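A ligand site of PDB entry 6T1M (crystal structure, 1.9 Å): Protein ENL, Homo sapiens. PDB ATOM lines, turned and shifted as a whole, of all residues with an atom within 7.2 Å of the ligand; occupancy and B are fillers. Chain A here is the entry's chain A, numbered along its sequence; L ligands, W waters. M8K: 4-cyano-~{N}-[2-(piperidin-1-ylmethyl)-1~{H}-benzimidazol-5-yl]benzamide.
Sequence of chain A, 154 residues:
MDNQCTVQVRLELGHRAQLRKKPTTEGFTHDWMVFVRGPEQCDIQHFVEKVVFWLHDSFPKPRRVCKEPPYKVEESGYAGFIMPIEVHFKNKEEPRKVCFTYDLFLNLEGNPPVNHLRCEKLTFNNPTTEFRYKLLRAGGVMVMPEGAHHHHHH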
ATOM      1  N   ARG A  20     -21.487 -19.999 -12.773  1.00  0.00           N
ATOM      2  CA  ARG A  20     -22.575 -20.814 -13.325  1.00  0.00           C
ATOM      3  C   ARG A  20     -22.062 -22.253 -13.439  1.00  0.00           C
ATOM      4  O   ARG A  20     -20.929 -22.403 -13.870  1.00  0.00           O
ATOM      5  CB  ARG A  20     -22.935 -20.166 -14.644  1.00  0.00           C
ATOM      6  CG  ARG A  20     -24.199 -20.656 -15.292  1.00  0.00           C
ATOM      7  CD  ARG A  20     -24.523 -19.798 -16.499  1.00  0.00           C
ATOM      8  NE  ARG A  20     -25.417 -20.497 -17.391  1.00  0.00           N
ATOM      9  CZ  ARG A  20     -26.717 -20.667 -17.173  1.00  0.00           C
ATOM     10  NH1 ARG A  20     -27.432 -21.394 -18.028  1.00  0.00           N
ATOM     11  NH2 ARG A  20     -27.311 -20.121 -16.133  1.00  0.00           N
ATOM     12  N   GLU A  26     -20.929 -23.884 -23.071  1.00  0.00           N
ATOM     13  CA  GLU A  26     -21.851 -22.743 -22.767  1.00  0.00           C
ATOM     14  C   GLU A  26     -21.001 -21.509 -22.414  1.00  0.00           C
ATOM     15  O   GLU A  26     -20.172 -21.624 -21.482  1.00  0.00           O
ATOM     16  CB  GLU A  26     -22.768 -23.145 -21.603  1.00  0.00           C
ATOM     17  CG  GLU A  26     -23.537 -21.997 -20.991  1.00  0.00           C
ATOM     18  CD  GLU A  26     -24.704 -21.505 -21.839  1.00  0.00           C
ATOM     19  OE1 GLU A  26     -24.683 -21.740 -23.112  1.00  0.00           O
ATOM     20  OE2 GLU A  26     -25.621 -20.897 -21.261  1.00  0.00           O
ATOM     21  N   PHE A  28     -21.446 -18.342 -21.172  1.00  0.00           N
ATOM     22  CA  PHE A  28     -21.695 -17.526 -19.964  1.00  0.00           C
ATOM     23  C   PHE A  28     -21.153 -18.245 -18.735  1.00  0.00           C
ATOM     24  O   PHE A  28     -21.600 -19.367 -18.434  1.00  0.00           O
ATOM     25  CB  PHE A  28     -23.183 -17.239 -19.825  1.00  0.00           C
ATOM     26  CG  PHE A  28     -23.809 -16.789 -21.109  1.00  0.00           C
ATOM     27  CD1 PHE A  28     -23.365 -15.638 -21.734  1.00  0.00           C
ATOM     28  CD2 PHE A  28     -24.773 -17.559 -21.748  1.00  0.00           C
ATOM     29  CE1 PHE A  28     -23.917 -15.227 -22.939  1.00  0.00           C
ATOM     30  CE2 PHE A  28     -25.337 -17.138 -22.940  1.00  0.00           C
ATOM     31  CZ  PHE A  28     -24.910 -15.965 -23.535  1.00  0.00           C
ATOM     32  N   HIS A  30     -21.316 -16.920 -15.577  1.00  0.00           N
ATOM     33  CA  HIS A  30     -21.922 -16.365 -14.335  1.00  0.00           C
ATOM     34  C   HIS A  30     -23.421 -16.273 -14.468  1.00  0.00           C
ATOM     35  O   HIS A  30     -23.915 -15.961 -15.553  1.00  0.00           O
ATOM     36  CB  HIS A  30     -21.342 -14.994 -14.011  1.00  0.00           C
ATOM     37  CG  HIS A  30     -19.958 -15.032 -13.442  1.00  0.00           C
ATOM     38  ND1 HIS A  30     -18.833 -15.139 -14.233  1.00  0.00           N
ATOM     39  CD2 HIS A  30     -19.517 -14.898 -12.166  1.00  0.00           C
ATOM     40  CE1 HIS A  30     -17.754 -15.059 -13.471  1.00  0.00           C
ATOM     41  NE2 HIS A  30     -18.142 -14.928 -12.203  1.00  0.00           N
ATOM     42  N   TRP A  32     -26.221 -13.757 -12.634  1.00  0.00           N
ATOM     43  CA  TRP A  32     -26.335 -12.556 -11.795  1.00  0.00           C
ATOM     44  C   TRP A  32     -27.752 -12.034 -11.754  1.00  0.00           C
ATOM     45  O   TRP A  32     -28.612 -12.453 -12.570  1.00  0.00           O
ATOM     46  CB  TRP A  32     -25.334 -11.468 -12.216  1.00  0.00           C
ATOM     47  CG  TRP A  32     -25.463 -11.023 -13.621  1.00  0.00           C
ATOM     48  CD1 TRP A  32     -24.593 -11.270 -14.645  1.00  0.00           C
ATOM     49  CD2 TRP A  32     -26.444 -10.125 -14.147  1.00  0.00           C
ATOM     50  NE1 TRP A  32     -25.005 -10.636 -15.780  1.00  0.00           N
ATOM     51  CE2 TRP A  32     -26.117  -9.899 -15.493  1.00  0.00           C
ATOM     52  CE3 TRP A  32     -27.560  -9.479 -13.602  1.00  0.00           C
ATOM     53  CZ2 TRP A  32     -26.875  -9.049 -16.311  1.00  0.00           C
ATOM     54  CZ3 TRP A  32     -28.321  -8.669 -14.404  1.00  0.00           C
ATOM     55  CH2 TRP A  32     -27.985  -8.457 -15.746  1.00  0.00           C
ATOM     56  N   HIS A  56     -26.089  -4.166 -20.896  1.00  0.00           N
ATOM     57  CA  HIS A  56     -25.116  -4.142 -22.005  1.00  0.00           C
ATOM     58  C   HIS A  56     -25.843  -4.369 -23.333  1.00  0.00           C
ATOM     59  O   HIS A  56     -26.768  -5.213 -23.342  1.00  0.00           O
ATOM     60  CB  HIS A  56     -24.036  -5.161 -21.727  1.00  0.00           C
ATOM     61  CG  HIS A  56     -22.836  -4.927 -22.559  1.00  0.00           C
ATOM     62  ND1 HIS A  56     -22.734  -5.386 -23.862  1.00  0.00           N
ATOM     63  CD2 HIS A  56     -21.692  -4.255 -22.297  1.00  0.00           C
ATOM     64  CE1 HIS A  56     -21.586  -5.009 -24.367  1.00  0.00           C
ATOM     65  NE2 HIS A  56     -20.905  -4.331 -23.414  1.00  0.00           N
ATOM     66  N   ASP A  57     -25.456  -3.626 -24.386  1.00  0.00           N
ATOM     67  CA  ASP A  57     -26.045  -3.632 -25.765  1.00  0.00           C
ATOM     68  C   ASP A  57     -26.069  -5.062 -26.321  1.00  0.00           C
ATOM     69  O   ASP A  57     -26.873  -5.325 -27.210  1.00  0.00           O
ATOM     70  CB  ASP A  57     -25.246  -2.736 -26.730  1.00  0.00           C
ATOM     71  CG  ASP A  57     -25.061  -1.285 -26.268  1.00  0.00           C
ATOM     72  OD1 ASP A  57     -24.993  -1.054 -25.038  1.00  0.00           O
ATOM     73  OD2 ASP A  57     -24.969  -0.390 -27.150  1.00  0.00           O
ATOM     74  N   SER A  58     -25.206  -5.935 -25.821  1.00  0.00           N
ATOM     75  CA  SER A  58     -25.022  -7.320 -26.309  1.00  0.00           C
ATOM     76  C   SER A  58     -26.193  -8.213 -25.886  1.00  0.00           C
ATOM     77  O   SER A  58     -26.326  -9.272 -26.462  1.00  0.00           O
ATOM     78  CB  SER A  58     -23.717  -7.896 -25.826  1.00  0.00           C
ATOM     79  OG  SER A  58     -23.787  -8.203 -24.448  1.00  0.00           O
ATOM     80  N   PHE A  59     -26.957  -7.838 -24.859  1.00  0.00           N
ATOM     81  CA  PHE A  59     -28.098  -8.662 -24.352  1.00  0.00           C
ATOM     82  C   PHE A  59     -29.286  -8.547 -25.291  1.00  0.00           C
ATOM     83  O   PHE A  59     -29.444  -7.549 -25.977  1.00  0.00           O
ATOM     84  CB  PHE A  59     -28.493  -8.250 -22.943  1.00  0.00           C
ATOM     85  CG  PHE A  59     -27.575  -8.732 -21.863  1.00  0.00           C
ATOM     86  CD1 PHE A  59     -26.455  -8.019 -21.509  1.00  0.00           C
ATOM     87  CD2 PHE A  59     -27.838  -9.918 -21.189  1.00  0.00           C
ATOM     88  CE1 PHE A  59     -25.646  -8.441 -20.475  1.00  0.00           C
ATOM     89  CE2 PHE A  59     -27.016 -10.347 -20.155  1.00  0.00           C
ATOM     90  CZ  PHE A  59     -25.911  -9.619 -19.813  1.00  0.00           C
ATOM     91  N   PRO A  60     -30.152  -9.574 -25.376  1.00  0.00           N
ATOM     92  CA  PRO A  60     -31.452  -9.424 -26.033  1.00  0.00           C
ATOM     93  C   PRO A  60     -32.344  -8.487 -25.191  1.00  0.00           C
ATOM     94  O   PRO A  60     -32.245  -8.542 -23.948  1.00  0.00           O
ATOM     95  CB  PRO A  60     -31.978 -10.859 -26.136  1.00  0.00           C
ATOM     96  CG  PRO A  60     -31.274 -11.602 -24.991  1.00  0.00           C
ATOM     97  CD  PRO A  60     -29.906 -10.946 -24.897  1.00  0.00           C
ATOM     98  N   ARG A  64     -34.739  -3.307 -19.963  1.00  0.00           N
ATOM     99  CA  ARG A  64     -35.569  -4.197 -19.105  1.00  0.00           C
ATOM    100  C   ARG A  64     -36.383  -3.329 -18.134  1.00  0.00           C
ATOM    101  O   ARG A  64     -35.776  -2.599 -17.343  1.00  0.00           O
ATOM    102  CB  ARG A  64     -34.693  -5.200 -18.363  1.00  0.00           C
ATOM    103  CG  ARG A  64     -33.830  -6.097 -19.257  1.00  0.00           C
ATOM    104  CD  ARG A  64     -34.617  -7.111 -20.083  1.00  0.00           C
ATOM    105  NE  ARG A  64     -33.743  -7.872 -20.956  1.00  0.00           N
ATOM    106  CZ  ARG A  64     -33.054  -8.959 -20.603  1.00  0.00           C
ATOM    107  NH1 ARG A  64     -32.257  -9.550 -21.478  1.00  0.00           N
ATOM    108  NH2 ARG A  64     -33.158  -9.473 -19.408  1.00  0.00           N
ATOM    109  N   GLU A  74     -32.746 -10.973 -13.678  1.00  0.00           N
ATOM    110  CA  GLU A  74     -31.889 -12.173 -13.528  1.00  0.00           C
ATOM    111  C   GLU A  74     -31.367 -12.539 -14.902  1.00  0.00           C
ATOM    112  O   GLU A  74     -32.185 -12.648 -15.813  1.00  0.00           O
ATOM    113  CB  GLU A  74     -32.663 -13.329 -12.911  1.00  0.00           C
ATOM    114  CG  GLU A  74     -33.022 -13.116 -11.448  1.00  0.00           C
ATOM    115  CD  GLU A  74     -34.175 -13.983 -10.945  1.00  0.00           C
ATOM    116  OE1 GLU A  74     -35.207 -14.126 -11.685  1.00  0.00           O
ATOM    117  OE2 GLU A  74     -34.038 -14.555  -9.825  1.00  0.00           O
ATOM    118  N   GLU A  75     -30.072 -12.751 -15.036  1.00  0.00           N
ATOM    119  CA  GLU A  75     -29.412 -13.001 -16.343  1.00  0.00           C
ATOM    120  C   GLU A  75     -28.214 -13.920 -16.143  1.00  0.00           C
ATOM    121  O   GLU A  75     -27.770 -14.119 -14.993  1.00  0.00           O
ATOM    122  CB  GLU A  75     -28.960 -11.685 -16.996  1.00  0.00           C
ATOM    123  CG  GLU A  75     -29.910 -11.168 -18.058  1.00  0.00           C
ATOM    124  CD  GLU A  75     -30.122 -12.054 -19.277  1.00  0.00           C
ATOM    125  OE1 GLU A  75     -29.434 -13.126 -19.388  1.00  0.00           O
ATOM    126  OE2 GLU A  75     -30.957 -11.676 -20.138  1.00  0.00           O
ATOM    127  N   SER A  76     -27.693 -14.417 -17.236  1.00  0.00           N
ATOM    128  CA  SER A  76     -26.369 -15.047 -17.304  1.00  0.00           C
ATOM    129  C   SER A  76     -25.462 -14.131 -18.123  1.00  0.00           C
ATOM    130  O   SER A  76     -26.000 -13.340 -18.901  1.00  0.00           O
ATOM    131  CB  SER A  76     -26.496 -16.399 -17.885  1.00  0.00           C
ATOM    132  OG  SER A  76     -27.217 -16.327 -19.096  1.00  0.00           O
ATOM    133  N   GLY A  77     -24.145 -14.183 -17.888  1.00  0.00           N
ATOM    134  CA  GLY A  77     -23.180 -13.388 -18.670  1.00  0.00           C
ATOM    135  C   GLY A  77     -21.737 -13.833 -18.446  1.00  0.00           C
ATOM    136  O   GLY A  77     -21.517 -14.774 -17.665  1.00  0.00           O
ATOM    137  N   TYR A  78     -20.796 -13.158 -19.088  1.00  0.00           N
ATOM    138  CA  TYR A  78     -19.351 -13.523 -19.094  1.00  0.00           C
ATOM    139  C   TYR A  78     -18.481 -12.339 -18.638  1.00  0.00           C
ATOM    140  O   TYR A  78     -17.256 -12.472 -18.730  1.00  0.00           O
ATOM    141  CB  TYR A  78     -18.912 -14.020 -20.479  1.00  0.00           C
ATOM    142  CG  TYR A  78     -19.294 -13.144 -21.659  1.00  0.00           C
ATOM    143  CD1 TYR A  78     -18.571 -12.011 -21.997  1.00  0.00           C
ATOM    144  CD2 TYR A  78     -20.352 -13.501 -22.480  1.00  0.00           C
ATOM    145  CE1 TYR A  78     -18.917 -11.244 -23.105  1.00  0.00           C
ATOM    146  CE2 TYR A  78     -20.731 -12.733 -23.571  1.00  0.00           C
ATOM    147  CZ  TYR A  78     -20.023 -11.592 -23.881  1.00  0.00           C
ATOM    148  OH  TYR A  78     -20.408 -10.874 -24.982  1.00  0.00           O
ATOM    149  N   ALA A  79     -19.086 -11.182 -18.314  1.00  0.00           N
ATOM    150  CA  ALA A  79     -18.359  -9.949 -17.914  1.00  0.00           C
ATOM    151  C   ALA A  79     -19.268  -9.008 -17.112  1.00  0.00           C
ATOM    152  O   ALA A  79     -20.487  -8.943 -17.396  1.00  0.00           O
ATOM    153  CB  ALA A  79     -17.809  -9.253 -19.135  1.00  0.00           C
ATOM    154  N   GLY A  80     -18.682  -8.279 -16.151  1.00  0.00           N
ATOM    155  CA  GLY A  80     -19.316  -7.129 -15.487  1.00  0.00           C
ATOM    156  C   GLY A  80     -19.534  -5.998 -16.466  1.00  0.00           C
ATOM    157  O   GLY A  80     -18.925  -6.020 -17.526  1.00  0.00           O
ATOM    158  N   PHE A  81     -20.350  -5.024 -16.118  1.00  0.00           N
ATOM    159  CA  PHE A  81     -20.520  -3.787 -16.906  1.00  0.00           C
ATOM    160  C   PHE A  81     -21.175  -2.717 -16.034  1.00  0.00           C
ATOM    161  O   PHE A  81     -21.645  -3.034 -14.954  1.00  0.00           O
ATOM    162  CB  PHE A  81     -21.329  -4.061 -18.187  1.00  0.00           C
ATOM    163  CG  PHE A  81     -22.690  -4.652 -17.957  1.00  0.00           C
ATOM    164  CD1 PHE A  81     -22.850  -6.015 -17.769  1.00  0.00           C
ATOM    165  CD2 PHE A  81     -23.815  -3.845 -17.888  1.00  0.00           C
ATOM    166  CE1 PHE A  81     -24.110  -6.572 -17.536  1.00  0.00           C
ATOM    167  CE2 PHE A  81     -25.072  -4.399 -17.672  1.00  0.00           C
ATOM    168  CZ  PHE A  81     -25.216  -5.765 -17.498  1.00  0.00           C
ATOM    169  N   ILE A  82     -21.135  -1.484 -16.498  1.00  0.00           N
ATOM    170  CA  ILE A  82     -21.844  -0.343 -15.887  1.00  0.00           C
ATOM    171  C   ILE A  82     -23.281  -0.335 -16.395  1.00  0.00           C
ATOM    172  O   ILE A  82     -23.496  -0.344 -17.644  1.00  0.00           O
ATOM    173  CB  ILE A  82     -21.128   0.968 -16.212  1.00  0.00           C
ATOM    174  CG1 ILE A  82     -19.673   0.939 -15.735  1.00  0.00           C
ATOM    175  CG2 ILE A  82     -21.902   2.128 -15.635  1.00  0.00           C
ATOM    176  CD1 ILE A  82     -19.501   0.478 -14.288  1.00  0.00           C
ATOM    177  N   LEU A 104     -22.233  -3.330 -12.015  1.00  0.00           N
ATOM    178  CA  LEU A 104     -22.462  -4.793 -12.027  1.00  0.00           C
ATOM    179  C   LEU A 104     -21.135  -5.511 -12.266  1.00  0.00           C
ATOM    180  O   LEU A 104     -20.851  -5.786 -13.402  1.00  0.00           O
ATOM    181  CB  LEU A 104     -23.467  -5.173 -13.116  1.00  0.00           C
ATOM    182  CG  LEU A 104     -24.042  -6.572 -12.941  1.00  0.00           C
ATOM    183  CD1 LEU A 104     -25.331  -6.519 -12.164  1.00  0.00           C
ATOM    184  CD2 LEU A 104     -24.243  -7.254 -14.257  1.00  0.00           C
ATOM    185  N   LEU A 106     -18.663  -9.023 -11.500  1.00  0.00           N
ATOM    186  CA  LEU A 106     -18.720 -10.484 -11.248  1.00  0.00           C
ATOM    187  C   LEU A 106     -17.602 -10.900 -10.283  1.00  0.00           C
ATOM    188  O   LEU A 106     -16.625 -10.168 -10.164  1.00  0.00           O
ATOM    189  CB  LEU A 106     -18.588 -11.214 -12.590  1.00  0.00           C
ATOM    190  CG  LEU A 106     -19.560 -10.731 -13.675  1.00  0.00           C
ATOM    191  CD1 LEU A 106     -19.489 -11.601 -14.911  1.00  0.00           C
ATOM    192  CD2 LEU A 106     -20.984 -10.683 -13.154  1.00  0.00           C
HETATM  193  N1  M8K L   1     -23.494 -10.372 -22.692  1.00  0.00           N
HETATM  194  C2  M8K L   1     -20.496  -7.421 -20.398  1.00  0.00           C
HETATM  195  N3  M8K L   1     -27.797 -13.819 -23.302  1.00  0.00           N
HETATM  196  C4  M8K L   1     -21.758  -9.066 -21.630  1.00  0.00           C
HETATM  197  N4  M8K L   1     -30.173 -14.768 -21.447  1.00  0.00           N
HETATM  198  C5  M8K L   1     -21.195  -8.590 -22.817  1.00  0.00           C
HETATM  199  C6  M8K L   1     -20.285  -7.549 -22.786  1.00  0.00           C
HETATM  200  O   M8K L   1     -22.600 -11.084 -20.725  1.00  0.00           O
HETATM  201  C7  M8K L   1     -22.665 -10.263 -21.629  1.00  0.00           C
HETATM  202  C3  M8K L   1     -21.406  -8.462 -20.429  1.00  0.00           C
HETATM  203  C1  M8K L   1     -19.925  -6.959 -21.580  1.00  0.00           C
HETATM  204  C   M8K L   1     -19.016  -5.838 -21.559  1.00  0.00           C
HETATM  205  N   M8K L   1     -18.302  -4.950 -21.585  1.00  0.00           N
HETATM  206  C8  M8K L   1     -24.596 -11.250 -22.852  1.00  0.00           C
HETATM  207  C13 M8K L   1     -25.061 -12.105 -21.841  1.00  0.00           C
HETATM  208  C12 M8K L   1     -26.165 -12.931 -22.105  1.00  0.00           C
HETATM  209  N2  M8K L   1     -26.870 -13.809 -21.267  1.00  0.00           N
HETATM  210  C14 M8K L   1     -27.832 -14.300 -22.033  1.00  0.00           C
HETATM  211  C11 M8K L   1     -26.748 -12.926 -23.367  1.00  0.00           C
HETATM  212  C10 M8K L   1     -26.299 -12.089 -24.378  1.00  0.00           C
HETATM  213  C9  M8K L   1     -25.225 -11.245 -24.111  1.00  0.00           C
HETATM  214  C15 M8K L   1     -28.833 -15.333 -21.596  1.00  0.00           C
HETATM  215  C20 M8K L   1     -30.736 -14.377 -22.765  1.00  0.00           C
HETATM  216  C19 M8K L   1     -32.259 -14.343 -22.782  1.00  0.00           C
HETATM  217  C18 M8K L   1     -32.815 -14.074 -21.421  1.00  0.00           C
HETATM  218  C17 M8K L   1     -32.435 -15.166 -20.467  1.00  0.00           C
HETATM  219  C16 M8K L   1     -31.075 -15.754 -20.813  1.00  0.00           C
HETATM  220  O   HOH W   1     -22.994 -10.109 -17.955  1.00  0.00           O
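A nitrogen (N1) of the ligand sits at hydrogen-bond distance from the side-chain hydroxyl of Ser 58 (2.8 Å).
The backbone NH (N) of Tyr 78 lies within hydrogen-bond range of an oxygen (O) of the ligand.
N2 of the ligand sits close to O of Ser 76, 2.6 Å away.
OG of Ser 76 lies close to N2 of the ligand (3.3 Å).
A ring nitrogen (NE2) of His 56 lies close to a nitrogen (N) of the ligand.
The side-chain carboxylate (OE1) of Glu 75 is in salt-bridge range of a nitrogen (N4) of the ligand, 2.7 Å away.
NH1 of Arg 64 lies within hydrogen-bond range of O of Pro 60, 2.7 Å away.
The backbone NH (N) of Phe 81 is in hydrogen-bond range of the backbone carbonyl oxygen (O) of Leu 104 (2.9 Å).
The side-chain carboxylate (OE2) of Glu 75 lies within salt-bridge range of the guanidinium group (NH1) of Arg 64, at 2.8 Å.
The backbone NH of Gly 77 is in hydrogen-bond range of the backbone carbonyl oxygen of His 30.
The side-chain hydroxyl (OG) of Ser 58 lies within hydrogen-bond range of a ring nitrogen (ND1) of His 56 (3.1 Å).
The backbone carbonyl oxygen (O) of Glu 75 is in hydrogen-bond range of the backbone NH (N) of Trp 32 (2.8 Å).
Residues that only touch the ligand: Phe 28, Phe 59, Pro 60, Gly 77, Ala 79, Gly 80 and Phe 81.
Of the 22 residues printed, 12 come within 4 Å of the ligand.
The nearest printed residue that does not touch the ligand is Arg 64 (4.6 Å).
Water W1 lies within hydrogen-bond range of O of Ala 79 (2.8 Å), O of the ligand (3.0 Å) and NE1 of Trp 32 (3.0 Å).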
